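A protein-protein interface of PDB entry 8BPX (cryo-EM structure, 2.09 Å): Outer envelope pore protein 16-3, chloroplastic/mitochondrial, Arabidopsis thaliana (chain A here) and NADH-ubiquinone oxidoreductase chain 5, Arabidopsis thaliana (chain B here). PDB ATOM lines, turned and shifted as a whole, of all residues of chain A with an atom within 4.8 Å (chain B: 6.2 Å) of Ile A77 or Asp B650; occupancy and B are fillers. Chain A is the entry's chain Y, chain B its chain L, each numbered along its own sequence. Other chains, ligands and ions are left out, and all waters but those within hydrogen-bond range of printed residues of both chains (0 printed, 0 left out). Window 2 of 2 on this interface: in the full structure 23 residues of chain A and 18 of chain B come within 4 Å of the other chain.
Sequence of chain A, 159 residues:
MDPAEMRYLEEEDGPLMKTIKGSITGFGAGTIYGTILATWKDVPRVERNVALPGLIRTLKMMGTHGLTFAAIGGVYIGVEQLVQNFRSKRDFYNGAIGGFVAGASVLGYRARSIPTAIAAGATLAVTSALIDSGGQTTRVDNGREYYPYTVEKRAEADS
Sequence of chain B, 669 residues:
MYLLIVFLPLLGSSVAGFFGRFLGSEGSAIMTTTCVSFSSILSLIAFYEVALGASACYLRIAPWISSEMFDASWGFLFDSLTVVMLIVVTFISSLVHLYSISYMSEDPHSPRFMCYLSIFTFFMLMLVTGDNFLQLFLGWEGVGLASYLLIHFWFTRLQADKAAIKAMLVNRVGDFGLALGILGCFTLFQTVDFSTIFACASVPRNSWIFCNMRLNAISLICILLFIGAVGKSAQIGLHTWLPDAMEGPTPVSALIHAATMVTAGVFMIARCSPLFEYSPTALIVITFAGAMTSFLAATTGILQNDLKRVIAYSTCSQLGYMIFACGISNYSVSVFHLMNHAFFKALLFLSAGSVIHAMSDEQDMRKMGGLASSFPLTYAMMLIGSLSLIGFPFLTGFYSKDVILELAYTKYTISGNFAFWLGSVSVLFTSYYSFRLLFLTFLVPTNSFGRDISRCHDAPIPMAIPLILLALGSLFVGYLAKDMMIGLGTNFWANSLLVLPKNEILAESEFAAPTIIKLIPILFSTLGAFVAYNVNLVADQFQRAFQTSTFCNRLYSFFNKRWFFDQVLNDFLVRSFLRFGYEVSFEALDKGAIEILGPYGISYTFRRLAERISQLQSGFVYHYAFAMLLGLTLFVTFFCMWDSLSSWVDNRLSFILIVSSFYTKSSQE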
ATOM      1  N   LYS A  18     -31.783   0.112  -9.213  1.00  0.00           N
ATOM      2  CA  LYS A  18     -30.736  -0.598  -8.487  1.00  0.00           C
ATOM      3  C   LYS A  18     -29.823  -1.353  -9.444  1.00  0.00           C
ATOM      4  O   LYS A  18     -28.597  -1.244  -9.363  1.00  0.00           O
ATOM      5  CB  LYS A  18     -31.358  -1.554  -7.469  1.00  0.00           C
ATOM      6  CG  LYS A  18     -32.069  -0.870  -6.313  1.00  0.00           C
ATOM      7  CD  LYS A  18     -31.106  -0.042  -5.485  1.00  0.00           C
ATOM      8  CE  LYS A  18     -31.721   0.343  -4.150  1.00  0.00           C
ATOM      9  NZ  LYS A  18     -30.840   1.258  -3.376  1.00  0.00           N
ATOM     10  N   THR A  19     -30.410  -2.111 -10.372  1.00  0.00           N
ATOM     11  CA  THR A  19     -29.606  -2.903 -11.299  1.00  0.00           C
ATOM     12  C   THR A  19     -28.787  -2.014 -12.231  1.00  0.00           C
ATOM     13  O   THR A  19     -27.601  -2.280 -12.467  1.00  0.00           O
ATOM     14  CB  THR A  19     -30.505  -3.841 -12.103  1.00  0.00           C
ATOM     15  OG1 THR A  19     -31.149  -4.764 -11.217  1.00  0.00           O
ATOM     16  CG2 THR A  19     -29.691  -4.617 -13.129  1.00  0.00           C
ATOM     17  N   GLY A  22     -26.007  -0.394 -10.269  1.00  0.00           N
ATOM     18  CA  GLY A  22     -25.002  -1.395  -9.965  1.00  0.00           C
ATOM     19  C   GLY A  22     -24.118  -1.702 -11.154  1.00  0.00           C
ATOM     20  O   GLY A  22     -22.905  -1.852 -11.009  1.00  0.00           O
ATOM     21  N   GLY A  73     -21.680  -6.596 -11.069  1.00  0.00           N
ATOM     22  CA  GLY A  73     -22.402  -5.611 -10.283  1.00  0.00           C
ATOM     23  C   GLY A  73     -23.844  -5.426 -10.695  1.00  0.00           C
ATOM     24  O   GLY A  73     -24.649  -4.937  -9.896  1.00  0.00           O
ATOM     25  N   GLY A  74     -24.186  -5.801 -11.922  1.00  0.00           N
ATOM     26  CA  GLY A  74     -25.559  -5.744 -12.364  1.00  0.00           C
ATOM     27  C   GLY A  74     -26.316  -7.015 -12.052  1.00  0.00           C
ATOM     28  O   GLY A  74     -27.406  -6.956 -11.479  1.00  0.00           O
ATOM     29  N   VAL A  75     -25.745  -8.166 -12.423  1.00  0.00           N
ATOM     30  CA  VAL A  75     -26.419  -9.443 -12.212  1.00  0.00           C
ATOM     31  C   VAL A  75     -26.645  -9.694 -10.724  1.00  0.00           C
ATOM     32  O   VAL A  75     -27.686 -10.229 -10.326  1.00  0.00           O
ATOM     33  CB  VAL A  75     -25.616 -10.580 -12.872  1.00  0.00           C
ATOM     34  CG1 VAL A  75     -25.842 -11.899 -12.152  1.00  0.00           C
ATOM     35  CG2 VAL A  75     -25.976 -10.699 -14.341  1.00  0.00           C
ATOM     36  N   TYR A  76     -25.688  -9.297  -9.878  1.00  0.00           N
ATOM     37  CA  TYR A  76     -25.834  -9.485  -8.438  1.00  0.00           C
ATOM     38  C   TYR A  76     -27.118  -8.846  -7.921  1.00  0.00           C
ATOM     39  O   TYR A  76     -28.006  -9.534  -7.401  1.00  0.00           O
ATOM     40  CB  TYR A  76     -24.612  -8.904  -7.725  1.00  0.00           C
ATOM     41  CG  TYR A  76     -24.669  -8.970  -6.221  1.00  0.00           C
ATOM     42  CD1 TYR A  76     -24.954 -10.160  -5.571  1.00  0.00           C
ATOM     43  CD2 TYR A  76     -24.431  -7.844  -5.451  1.00  0.00           C
ATOM     44  CE1 TYR A  76     -25.001 -10.224  -4.193  1.00  0.00           C
ATOM     45  CE2 TYR A  76     -24.474  -7.898  -4.076  1.00  0.00           C
ATOM     46  CZ  TYR A  76     -24.762  -9.090  -3.451  1.00  0.00           C
ATOM     47  OH  TYR A  76     -24.809  -9.147  -2.077  1.00  0.00           O
ATOM     48  N   ILE A  77     -27.238  -7.526  -8.073  1.00  0.00           N
ATOM     49  CA  ILE A  77     -28.417  -6.825  -7.578  1.00  0.00           C
ATOM     50  C   ILE A  77     -29.666  -7.252  -8.334  1.00  0.00           C
ATOM     51  O   ILE A  77     -30.749  -7.329  -7.746  1.00  0.00           O
ATOM     52  CB  ILE A  77     -28.210  -5.302  -7.647  1.00  0.00           C
ATOM     53  CG1 ILE A  77     -27.104  -4.877  -6.680  1.00  0.00           C
ATOM     54  CG2 ILE A  77     -29.522  -4.573  -7.361  1.00  0.00           C
ATOM     55  CD1 ILE A  77     -26.636  -3.445  -6.854  1.00  0.00           C
ATOM     56  N   GLY A  78     -29.553  -7.540  -9.631  1.00  0.00           N
ATOM     57  CA  GLY A  78     -30.726  -7.946 -10.385  1.00  0.00           C
ATOM     58  C   GLY A  78     -31.330  -9.236  -9.869  1.00  0.00           C
ATOM     59  O   GLY A  78     -32.536  -9.319  -9.635  1.00  0.00           O
ATOM     60  N   VAL A  79     -30.495 -10.256  -9.666  1.00  0.00           N
ATOM     61  CA  VAL A  79     -30.999 -11.519  -9.143  1.00  0.00           C
ATOM     62  C   VAL A  79     -31.441 -11.351  -7.696  1.00  0.00           C
ATOM     63  O   VAL A  79     -32.435 -11.950  -7.267  1.00  0.00           O
ATOM     64  CB  VAL A  79     -29.946 -12.629  -9.297  1.00  0.00           C
ATOM     65  CG1 VAL A  79     -30.377 -13.874  -8.536  1.00  0.00           C
ATOM     66  CG2 VAL A  79     -29.730 -12.947 -10.764  1.00  0.00           C
ATOM     67  N   GLU A  80     -30.732 -10.520  -6.925  1.00  0.00           N
ATOM     68  CA  GLU A  80     -31.138 -10.271  -5.546  1.00  0.00           C
ATOM     69  C   GLU A  80     -32.547  -9.696  -5.479  1.00  0.00           C
ATOM     70  O   GLU A  80     -33.379 -10.148  -4.684  1.00  0.00           O
ATOM     71  CB  GLU A  80     -30.143  -9.326  -4.876  1.00  0.00           C
ATOM     72  CG  GLU A  80     -30.600  -8.811  -3.521  1.00  0.00           C
ATOM     73  CD  GLU A  80     -29.775  -7.639  -3.037  1.00  0.00           C
ATOM     74  OE1 GLU A  80     -28.706  -7.379  -3.628  1.00  0.00           O
ATOM     75  OE2 GLU A  80     -30.193  -6.977  -2.064  1.00  0.00           O
ATOM     76  N   GLN A  81     -32.834  -8.695  -6.313  1.00  0.00           N
ATOM     77  CA  GLN A  81     -34.158  -8.083  -6.300  1.00  0.00           C
ATOM     78  C   GLN A  81     -35.200  -9.011  -6.910  1.00  0.00           C
ATOM     79  O   GLN A  81     -36.336  -9.078  -6.427  1.00  0.00           O
ATOM     80  CB  GLN A  81     -34.127  -6.742  -7.033  1.00  0.00           C
ATOM     81  CG  GLN A  81     -33.097  -5.743  -6.509  1.00  0.00           C
ATOM     82  CD  GLN A  81     -33.313  -5.335  -5.061  1.00  0.00           C
ATOM     83  OE1 GLN A  81     -33.190  -6.146  -4.142  1.00  0.00           O
ATOM     84  NE2 GLN A  81     -33.630  -4.062  -4.850  1.00  0.00           N
ATOM     85  N   LEU A  82     -34.832  -9.744  -7.963  1.00  0.00           N
ATOM     86  CA  LEU A  82     -35.736 -10.716  -8.562  1.00  0.00           C
ATOM     87  C   LEU A  82     -36.010 -11.900  -7.645  1.00  0.00           C
ATOM     88  O   LEU A  82     -36.925 -12.681  -7.926  1.00  0.00           O
ATOM     89  CB  LEU A  82     -35.160 -11.208  -9.890  1.00  0.00           C
ATOM     90  CG  LEU A  82     -36.153 -11.410 -11.036  1.00  0.00           C
ATOM     91  CD1 LEU A  82     -37.260 -10.370 -10.978  1.00  0.00           C
ATOM     92  CD2 LEU A  82     -35.440 -11.367 -12.379  1.00  0.00           C
ATOM     93  N   LEU B 645     -21.474   9.513  -3.310  1.00  0.00           N
ATOM     94  CA  LEU B 645     -21.296   8.163  -3.908  1.00  0.00           C
ATOM     95  C   LEU B 645     -22.544   7.329  -3.636  1.00  0.00           C
ATOM     96  O   LEU B 645     -23.041   6.654  -4.556  1.00  0.00           O
ATOM     97  CB  LEU B 645     -20.045   7.515  -3.304  1.00  0.00           C
ATOM     98  CG  LEU B 645     -18.721   8.208  -3.630  1.00  0.00           C
ATOM     99  CD1 LEU B 645     -17.573   7.572  -2.865  1.00  0.00           C
ATOM    100  CD2 LEU B 645     -18.435   8.183  -5.125  1.00  0.00           C
ATOM    101  N   SER B 646     -23.017   7.385  -2.401  1.00  0.00           N
ATOM    102  CA  SER B 646     -23.975   6.422  -1.868  1.00  0.00           C
ATOM    103  C   SER B 646     -25.244   6.361  -2.709  1.00  0.00           C
ATOM    104  O   SER B 646     -26.004   5.390  -2.625  1.00  0.00           O
ATOM    105  CB  SER B 646     -24.322   6.764  -0.419  1.00  0.00           C
ATOM    106  OG  SER B 646     -23.171   6.724   0.407  1.00  0.00           O
ATOM    107  N   TRP B 648     -25.382   6.197  -6.101  1.00  0.00           N
ATOM    108  CA  TRP B 648     -25.163   5.136  -7.118  1.00  0.00           C
ATOM    109  C   TRP B 648     -24.715   3.835  -6.438  1.00  0.00           C
ATOM    110  O   TRP B 648     -25.037   2.757  -6.972  1.00  0.00           O
ATOM    111  CB  TRP B 648     -24.147   5.605  -8.160  1.00  0.00           C
ATOM    112  CG  TRP B 648     -24.734   6.313  -9.340  1.00  0.00           C
ATOM    113  CD1 TRP B 648     -24.861   5.826 -10.608  1.00  0.00           C
ATOM    114  CD2 TRP B 648     -25.243   7.657  -9.373  1.00  0.00           C
ATOM    115  NE1 TRP B 648     -25.429   6.767 -11.423  1.00  0.00           N
ATOM    116  CE2 TRP B 648     -25.673   7.901 -10.694  1.00  0.00           C
ATOM    117  CE3 TRP B 648     -25.387   8.670  -8.420  1.00  0.00           C
ATOM    118  CZ2 TRP B 648     -26.237   9.115 -11.080  1.00  0.00           C
ATOM    119  CZ3 TRP B 648     -25.943   9.870  -8.802  1.00  0.00           C
ATOM    120  CH2 TRP B 648     -26.360  10.088 -10.115  1.00  0.00           C
ATOM    121  N   VAL B 649     -24.011   3.939  -5.308  1.00  0.00           N
ATOM    122  CA  VAL B 649     -23.168   2.821  -4.788  1.00  0.00           C
ATOM    123  C   VAL B 649     -23.823   2.205  -3.546  1.00  0.00           C
ATOM    124  O   VAL B 649     -24.583   2.898  -2.838  1.00  0.00           O
ATOM    125  CB  VAL B 649     -21.717   3.247  -4.496  1.00  0.00           C
ATOM    126  CG1 VAL B 649     -21.149   4.150  -5.580  1.00  0.00           C
ATOM    127  CG2 VAL B 649     -21.538   3.862  -3.117  1.00  0.00           C
ATOM    128  N   ASP B 650     -23.532   0.924  -3.342  1.00  0.00           N
ATOM    129  CA  ASP B 650     -23.878   0.110  -2.163  1.00  0.00           C
ATOM    130  C   ASP B 650     -22.608  -0.594  -1.585  1.00  0.00           C
ATOM    131  O   ASP B 650     -21.722  -1.168  -2.406  1.00  0.00           O
ATOM    132  CB  ASP B 650     -24.495  -1.248  -2.530  1.00  0.00           C
ATOM    133  CG  ASP B 650     -25.769  -1.152  -3.349  1.00  0.00           C
ATOM    134  OD1 ASP B 650     -25.726  -0.538  -4.432  1.00  0.00           O
ATOM    135  OD2 ASP B 650     -26.794  -1.700  -2.898  1.00  0.00           O
ATOM    136  N   ASN B 651     -22.611  -0.881  -0.274  1.00  0.00           N
ATOM    137  CA  ASN B 651     -21.465  -1.526   0.422  1.00  0.00           C
ATOM    138  C   ASN B 651     -21.350  -2.995  -0.014  1.00  0.00           C
ATOM    139  O   ASN B 651     -20.200  -3.509  -0.263  1.00  0.00           O
ATOM    140  CB  ASN B 651     -21.562  -1.372   1.941  1.00  0.00           C
ATOM    141  CG  ASN B 651     -21.310   0.043   2.417  1.00  0.00           C
ATOM    142  OD1 ASN B 651     -20.665   0.826   1.724  1.00  0.00           O
ATOM    143  ND2 ASN B 651     -21.813   0.380   3.596  1.00  0.00           N
ATOM    144  N   ARG B 652     -22.498  -3.583  -0.263  1.00  0.00           N
ATOM    145  CA  ARG B 652     -22.513  -4.989  -0.739  1.00  0.00           C
ATOM    146  C   ARG B 652     -21.664  -5.101  -2.011  1.00  0.00           C
ATOM    147  O   ARG B 652     -20.689  -5.907  -2.017  1.00  0.00           O
ATOM    148  CB  ARG B 652     -23.962  -5.316  -1.061  1.00  0.00           C
ATOM    149  CG  ARG B 652     -24.967  -4.641  -0.138  1.00  0.00           C
ATOM    150  CD  ARG B 652     -25.530  -5.618   0.873  1.00  0.00           C
ATOM    151  NE  ARG B 652     -25.869  -6.879   0.237  1.00  0.00           N
ATOM    152  CZ  ARG B 652     -27.028  -7.129  -0.362  1.00  0.00           C
ATOM    153  NH1 ARG B 652     -27.970  -6.202  -0.400  1.00  0.00           N
ATOM    154  NH2 ARG B 652     -27.243  -8.307  -0.916  1.00  0.00           N
ATOM    155  N   LEU B 653     -21.994  -4.295  -3.013  1.00  0.00           N
ATOM    156  CA  LEU B 653     -21.314  -4.349  -4.315  1.00  0.00           C
ATOM    157  C   LEU B 653     -19.816  -4.035  -4.069  1.00  0.00           C
ATOM    158  O   LEU B 653     -19.025  -4.793  -4.569  1.00  0.00           O
ATOM    159  CB  LEU B 653     -21.929  -3.363  -5.311  1.00  0.00           C
ATOM    160  CG  LEU B 653     -23.362  -3.658  -5.760  1.00  0.00           C
ATOM    161  CD1 LEU B 653     -23.895  -2.528  -6.627  1.00  0.00           C
ATOM    162  CD2 LEU B 653     -23.432  -4.986  -6.499  1.00  0.00           C
ATOM    163  N   SER B 654     -19.487  -3.004  -3.296  1.00  0.00           N
ATOM    164  CA  SER B 654     -18.074  -2.716  -2.942  1.00  0.00           C
ATOM    165  C   SER B 654     -17.360  -4.019  -2.596  1.00  0.00           C
ATOM    166  O   SER B 654     -16.447  -4.399  -3.349  1.00  0.00           O
ATOM    167  CB  SER B 654     -17.968  -1.702  -1.826  1.00  0.00           C
ATOM    168  OG  SER B 654     -16.701  -1.775  -1.188  1.00  0.00           O
ATOM    169  N   PHE B 655     -17.789  -4.744  -1.567  1.00  0.00           N
ATOM    170  CA  PHE B 655     -16.941  -5.859  -1.078  1.00  0.00           C
ATOM    171  C   PHE B 655     -17.022  -7.045  -2.056  1.00  0.00           C
ATOM    172  O   PHE B 655     -16.013  -7.754  -2.203  1.00  0.00           O
ATOM    173  CB  PHE B 655     -17.319  -6.230   0.358  1.00  0.00           C
ATOM    174  CG  PHE B 655     -16.690  -5.355   1.410  1.00  0.00           C
ATOM    175  CD1 PHE B 655     -15.375  -5.549   1.798  1.00  0.00           C
ATOM    176  CD2 PHE B 655     -17.409  -4.331   2.005  1.00  0.00           C
ATOM    177  CE1 PHE B 655     -14.795  -4.743   2.764  1.00  0.00           C
ATOM    178  CE2 PHE B 655     -16.826  -3.525   2.969  1.00  0.00           C
ATOM    179  CZ  PHE B 655     -15.521  -3.733   3.348  1.00  0.00           C
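The guanidinium group (NH2) of Arg B652 sits at hydrogen-bond distance from the side-chain hydroxyl (OH) of Tyr A76 (2.8 Å).
NH1 of Arg B652 lies within salt-bridge range of OE2 of Glu A80 (2.9 Å).
Gly A22 touches Leu B653.
Gly A73 touches Leu B653 (O to CD2, 3.6 Å).
Tyr A76 touches Leu B653.
Asp B650 touches Ile A77 (OD1 to CD1, 3.9 Å).
Leu B653 touches Ile A77 (CD1 to CD1, 2.9 Å).
Of chain B, only Asp B650 and Leu B653 come within 4 Å of Ile A77.
Printed residues of chain A within 4 Å of Asp B650: Ile A77 (3.9 Å).
Of the printed residues of chain B, Gly A22 touches Leu B653 (3.7 Å).
Of the printed residues of chain A, Arg B652 touches Tyr A76 (2.8 Å) and Glu A80 (2.9 Å).
Of the printed residues of chain B, Gly A73 touches Leu B653.
The nearest printed residue of chain B that does not touch Ile A77 is Trp B648 (6.4 Å).
The nearest printed residue of chain A that does not touch Asp B650 is Lys A18 (5.0 Å).
The nearest printed residue of chain B that does not touch Gly A22 is Trp B648 (4.7 Å).
Of the 10 printed residues of chain B, 3 touch a printed residue of chain A.
Printed residues of chain B that touch a printed residue of chain A: Asp B650, Arg B652 and Leu B653.
Hydrophobic or aromatic side chains of chain B within 4 Å of the printed part of chain A: Leu B653.
Of the 13 printed residues of chain A, 5 touch a printed residue of chain B.
Printed residues of chain A that touch a printed residue of chain B: Gly A22, Gly A73, Tyr A76, Ile A77 and Glu A80.
Hydrophobic or aromatic side chains of chain A within 4 Å of the printed part of chain B: Tyr A76 and Ile A77.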
